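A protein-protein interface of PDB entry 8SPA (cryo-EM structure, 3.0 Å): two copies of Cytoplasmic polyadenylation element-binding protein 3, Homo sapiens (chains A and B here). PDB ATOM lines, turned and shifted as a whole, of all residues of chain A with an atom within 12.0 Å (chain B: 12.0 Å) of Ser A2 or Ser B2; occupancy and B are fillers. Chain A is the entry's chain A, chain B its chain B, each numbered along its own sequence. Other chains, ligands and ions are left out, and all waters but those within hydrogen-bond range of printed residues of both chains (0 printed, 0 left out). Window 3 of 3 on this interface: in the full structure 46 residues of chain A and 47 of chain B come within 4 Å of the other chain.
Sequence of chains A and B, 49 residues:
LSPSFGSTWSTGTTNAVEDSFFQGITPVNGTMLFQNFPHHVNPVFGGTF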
ATOM      1  N   LEU A   1     -13.506   1.756  12.393  1.00  0.00           N
ATOM      2  CA  LEU A   1     -13.744   1.967  10.969  1.00  0.00           C
ATOM      3  C   LEU A   1     -12.441   1.958  10.175  1.00  0.00           C
ATOM      4  O   LEU A   1     -11.508   2.700  10.473  1.00  0.00           O
ATOM      5  CB  LEU A   1     -14.514   3.274  10.741  1.00  0.00           C
ATOM      6  CG  LEU A   1     -13.858   4.641  10.941  1.00  0.00           C
ATOM      7  CD1 LEU A   1     -14.696   5.718  10.287  1.00  0.00           C
ATOM      8  CD2 LEU A   1     -13.695   4.938  12.418  1.00  0.00           C
ATOM      9  N   SER A   2     -12.379   1.092   9.167  1.00  0.00           N
ATOM     10  CA  SER A   2     -11.169   0.916   8.364  1.00  0.00           C
ATOM     11  C   SER A   2     -11.560   0.557   6.942  1.00  0.00           C
ATOM     12  O   SER A   2     -11.474  -0.604   6.525  1.00  0.00           O
ATOM     13  CB  SER A   2     -10.264  -0.159   8.962  1.00  0.00           C
ATOM     14  OG  SER A   2     -10.980  -1.364   9.164  1.00  0.00           O
ATOM     15  N   PRO A   3     -12.006   1.535   6.162  1.00  0.00           N
ATOM     16  CA  PRO A   3     -12.350   1.262   4.765  1.00  0.00           C
ATOM     17  C   PRO A   3     -11.125   0.869   3.959  1.00  0.00           C
ATOM     18  O   PRO A   3     -10.008   1.322   4.217  1.00  0.00           O
ATOM     19  CB  PRO A   3     -12.930   2.592   4.272  1.00  0.00           C
ATOM     20  CG  PRO A   3     -13.239   3.367   5.510  1.00  0.00           C
ATOM     21  CD  PRO A   3     -12.232   2.942   6.516  1.00  0.00           C
ATOM     22  N   SER A   4     -11.349   0.012   2.969  1.00  0.00           N
ATOM     23  CA  SER A   4     -10.303  -0.427   2.058  1.00  0.00           C
ATOM     24  C   SER A   4     -10.695  -0.026   0.646  1.00  0.00           C
ATOM     25  O   SER A   4     -11.766  -0.409   0.166  1.00  0.00           O
ATOM     26  CB  SER A   4     -10.094  -1.938   2.148  1.00  0.00           C
ATOM     27  OG  SER A   4      -9.108  -2.366   1.227  1.00  0.00           O
ATOM     28  N   PHE A   5      -9.836   0.738  -0.014  1.00  0.00           N
ATOM     29  CA  PHE A   5     -10.094   1.212  -1.364  1.00  0.00           C
ATOM     30  C   PHE A   5      -9.211   0.456  -2.348  1.00  0.00           C
ATOM     31  O   PHE A   5      -8.262  -0.233  -1.970  1.00  0.00           O
ATOM     32  CB  PHE A   5      -9.853   2.718  -1.473  1.00  0.00           C
ATOM     33  CG  PHE A   5     -10.789   3.550  -0.647  1.00  0.00           C
ATOM     34  CD1 PHE A   5     -11.829   2.975   0.052  1.00  0.00           C
ATOM     35  CD2 PHE A   5     -10.625   4.916  -0.573  1.00  0.00           C
ATOM     36  CE1 PHE A   5     -12.676   3.743   0.811  1.00  0.00           C
ATOM     37  CE2 PHE A   5     -11.472   5.685   0.185  1.00  0.00           C
ATOM     38  CZ  PHE A   5     -12.499   5.100   0.874  1.00  0.00           C
ATOM     39  N   GLY A   6      -9.530   0.603  -3.633  1.00  0.00           N
ATOM     40  CA  GLY A   6      -8.776  -0.018  -4.695  1.00  0.00           C
ATOM     41  C   GLY A   6      -7.983   1.006  -5.486  1.00  0.00           C
ATOM     42  O   GLY A   6      -8.196   2.216  -5.382  1.00  0.00           O
ATOM     43  N   GLN A  23      -9.059  13.384  -1.634  1.00  0.00           N
ATOM     44  CA  GLN A  23      -8.821  12.022  -1.185  1.00  0.00           C
ATOM     45  C   GLN A  23      -8.387  12.045   0.270  1.00  0.00           C
ATOM     46  O   GLN A  23      -7.665  12.950   0.693  1.00  0.00           O
ATOM     47  CB  GLN A  23      -7.761  11.336  -2.045  1.00  0.00           C
ATOM     48  CG  GLN A  23      -7.701   9.842  -1.860  1.00  0.00           C
ATOM     49  CD  GLN A  23      -7.112   9.133  -3.056  1.00  0.00           C
ATOM     50  OE1 GLN A  23      -6.764   9.762  -4.052  1.00  0.00           O
ATOM     51  NE2 GLN A  23      -6.990   7.817  -2.963  1.00  0.00           N
ATOM     52  N   GLY A  24      -8.828  11.054   1.032  1.00  0.00           N
ATOM     53  CA  GLY A  24      -8.476  10.957   2.435  1.00  0.00           C
ATOM     54  C   GLY A  24      -9.474  11.666   3.326  1.00  0.00           C
ATOM     55  O   GLY A  24     -10.450  12.274   2.877  1.00  0.00           O
ATOM     56  N   ILE A  25      -9.202  11.583   4.626  1.00  0.00           N
ATOM     57  CA  ILE A  25     -10.094  12.153   5.629  1.00  0.00           C
ATOM     58  C   ILE A  25     -10.159  13.660   5.437  1.00  0.00           C
ATOM     59  O   ILE A  25      -9.163  14.367   5.623  1.00  0.00           O
ATOM     60  CB  ILE A  25      -9.625  11.797   7.044  1.00  0.00           C
ATOM     61  CG1 ILE A  25      -9.692  10.287   7.270  1.00  0.00           C
ATOM     62  CG2 ILE A  25     -10.465  12.511   8.074  1.00  0.00           C
ATOM     63  CD1 ILE A  25      -8.409   9.566   6.960  1.00  0.00           C
ATOM     64  N   THR A  26     -11.333  14.160   5.065  1.00  0.00           N
ATOM     65  CA  THR A  26     -11.535  15.577   4.768  1.00  0.00           C
ATOM     66  C   THR A  26     -12.788  16.081   5.474  1.00  0.00           C
ATOM     67  O   THR A  26     -13.818  16.321   4.832  1.00  0.00           O
ATOM     68  CB  THR A  26     -11.638  15.806   3.261  1.00  0.00           C
ATOM     69  OG1 THR A  26     -10.639  15.027   2.591  1.00  0.00           O
ATOM     70  CG2 THR A  26     -11.440  17.270   2.926  1.00  0.00           C
ATOM     71  N   LEU B   1      -9.571   4.704  13.234  1.00  0.00           N
ATOM     72  CA  LEU B   1      -9.773   4.850  11.796  1.00  0.00           C
ATOM     73  C   LEU B   1      -8.450   4.802  11.036  1.00  0.00           C
ATOM     74  O   LEU B   1      -7.523   5.555  11.324  1.00  0.00           O
ATOM     75  CB  LEU B   1     -10.533   6.146  11.489  1.00  0.00           C
ATOM     76  CG  LEU B   1      -9.879   7.519  11.643  1.00  0.00           C
ATOM     77  CD1 LEU B   1     -10.697   8.567  10.919  1.00  0.00           C
ATOM     78  CD2 LEU B   1      -9.753   7.883  13.109  1.00  0.00           C
ATOM     79  N   SER B   2      -8.365   3.891  10.072  1.00  0.00           N
ATOM     80  CA  SER B   2      -7.136   3.675   9.307  1.00  0.00           C
ATOM     81  C   SER B   2      -7.494   3.253   7.894  1.00  0.00           C
ATOM     82  O   SER B   2      -7.400   2.073   7.533  1.00  0.00           O
ATOM     83  CB  SER B   2      -6.249   2.628   9.976  1.00  0.00           C
ATOM     84  OG  SER B   2      -6.973   1.435  10.217  1.00  0.00           O
ATOM     85  N   PRO B   3      -7.917   4.195   7.059  1.00  0.00           N
ATOM     86  CA  PRO B   3      -8.227   3.858   5.669  1.00  0.00           C
ATOM     87  C   PRO B   3      -6.984   3.426   4.913  1.00  0.00           C
ATOM     88  O   PRO B   3      -5.873   3.889   5.178  1.00  0.00           O
ATOM     89  CB  PRO B   3      -8.790   5.165   5.101  1.00  0.00           C
ATOM     90  CG  PRO B   3      -9.129   5.996   6.293  1.00  0.00           C
ATOM     91  CD  PRO B   3      -8.148   5.617   7.343  1.00  0.00           C
ATOM     92  N   SER B   4      -7.185   2.526   3.957  1.00  0.00           N
ATOM     93  CA  SER B   4      -6.117   2.043   3.094  1.00  0.00           C
ATOM     94  C   SER B   4      -6.473   2.379   1.656  1.00  0.00           C
ATOM     95  O   SER B   4      -7.533   1.976   1.167  1.00  0.00           O
ATOM     96  CB  SER B   4      -5.915   0.537   3.258  1.00  0.00           C
ATOM     97  OG  SER B   4      -4.907   0.067   2.383  1.00  0.00           O
ATOM     98  N   PHE B   5      -5.596   3.111   0.983  1.00  0.00           N
ATOM     99  CA  PHE B   5      -5.818   3.523  -0.394  1.00  0.00           C
ATOM    100  C   PHE B   5      -4.914   2.723  -1.320  1.00  0.00           C
ATOM    101  O   PHE B   5      -3.977   2.048  -0.887  1.00  0.00           O
ATOM    102  CB  PHE B   5      -5.572   5.022  -0.566  1.00  0.00           C
ATOM    103  CG  PHE B   5      -6.526   5.893   0.197  1.00  0.00           C
ATOM    104  CD1 PHE B   5      -7.584   5.351   0.895  1.00  0.00           C
ATOM    105  CD2 PHE B   5      -6.360   7.260   0.212  1.00  0.00           C
ATOM    106  CE1 PHE B   5      -8.448   6.155   1.597  1.00  0.00           C
ATOM    107  CE2 PHE B   5      -7.224   8.065   0.913  1.00  0.00           C
ATOM    108  CZ  PHE B   5      -8.269   7.513   1.604  1.00  0.00           C
ATOM    109  N   GLY B   6      -5.201   2.810  -2.618  1.00  0.00           N
ATOM    110  CA  GLY B   6      -4.422   2.139  -3.631  1.00  0.00           C
ATOM    111  C   GLY B   6      -3.607   3.125  -4.448  1.00  0.00           C
ATOM    112  O   GLY B   6      -3.820   4.338  -4.404  1.00  0.00           O
ATOM    113  N   GLY B  24      -4.588  13.463   1.578  1.00  0.00           N
ATOM    114  CA  GLY B  24      -4.271  13.431   2.991  1.00  0.00           C
ATOM    115  C   GLY B  24      -5.290  14.181   3.825  1.00  0.00           C
ATOM    116  O   GLY B  24      -6.252  14.769   3.324  1.00  0.00           O
ATOM    117  N   ILE B  25      -5.051  14.157   5.133  1.00  0.00           N
ATOM    118  CA  ILE B  25      -5.965  14.774   6.087  1.00  0.00           C
ATOM    119  C   ILE B  25      -6.022  16.272   5.824  1.00  0.00           C
ATOM    120  O   ILE B  25      -5.029  16.985   6.002  1.00  0.00           O
ATOM    121  CB  ILE B  25      -5.533  14.482   7.528  1.00  0.00           C
ATOM    122  CG1 ILE B  25      -5.609  12.986   7.821  1.00  0.00           C
ATOM    123  CG2 ILE B  25      -6.396  15.246   8.503  1.00  0.00           C
ATOM    124  CD1 ILE B  25      -4.320  12.249   7.576  1.00  0.00           C
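Hydrophobic or aromatic side chains of chain B that line the printed part of chain A: Leu B1, Pro B3 and Phe B5. Along chain B the printed residues that touch a printed residue of chain A span positions 1 to 25. Hydrophobic or aromatic side chains of chain A that line the printed part of chain B: Leu A1, Phe A5 and Ile A25. Along chain A the printed residues that touch a printed residue of chain B span positions 1 to 25.
The backbone carbonyl oxygen (O) of Leu A1 is in hydrogen-bond range of the backbone NH (N) of Ser B2 (3.4 Å). N of Ser B4 sits at hydrogen-bond distance from O of Pro A3 (3.1 Å). The backbone carbonyl oxygen (O) of Ser B4 sits at hydrogen-bond distance from the backbone NH (N) of Phe A5 (2.9 Å). O of Gln A23 is in hydrogen-bond range of N of Gly B24.
CA of Leu B1 touches O of Leu A1, 3.1 Å away. OG of Ser B2 touches CB of Ser A2 (3.9 Å). O of Pro A3 touches CA of Pro B3, at 3.4 Å. Ser B4 touches Ser A4 (O to CA, 3.8 Å). CE1 of Phe B5 touches CD2 of Phe A5, 3.3 Å away. CD2 of Phe B5 touches NE2 of Gln A23 (3.3 Å). N of Gly A24 touches CE2 of Phe B5 (3.4 Å). Pro B3 touches Ile A25. Ile A25 touches Gly B24. Ile B25 touches Ile A25 (CA to O, 3.3 Å).
OG1 of Thr A26 sits at hydrogen-bond distance from O of Gly A24.
Of chain B, only Pro B3 (3.4 Å) and Ser B4 (3.1 Å) come within 4 Å of Pro A3. Ser A4 touches just one residue of chain B: Ser B4. Printed residues of chain B within 4 Å of Phe A5: Ser B4 (2.9 Å) and Phe B5 (3.3 Å). Printed residues of chain B within 4 Å of Gln A23: Phe B5 (3.3 Å) and Gly B24 (3.2 Å). Of the printed residues of chain B, Ile A25 touches Pro B3 (3.7 Å), Gly B24 (3.7 Å) and Ile B25 (3.3 Å). Ser B2 touches just these residues of chain A: Leu A1 (3.4 Å) and Ser A2 (3.9 Å). Pro B3 touches two residues of chain A. Printed residues of chain A within 4 Å of Phe B5: Phe A5, Gln A23 and Gly A24. Gly B6 touches none of the printed residues of chain A. Of the printed residues of chain A, Ile B25 touches Ile A25.
Ser A2 touches its own counterpart, Ser B2. Ser A4 touches its own counterpart, Ser B4. Ile A25 touches Pro B3, but with the chains exchanged Pro A3 does not touch Ile B25 (12.1 Å). Ile A25 touches Gly B24, but with the chains exchanged Gly A24 does not touch Ile B25 (5.4 Å). Of the 14 pairs that touch across the chains among the printed residues, 6 have their exchanged pair printed and touching as well.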
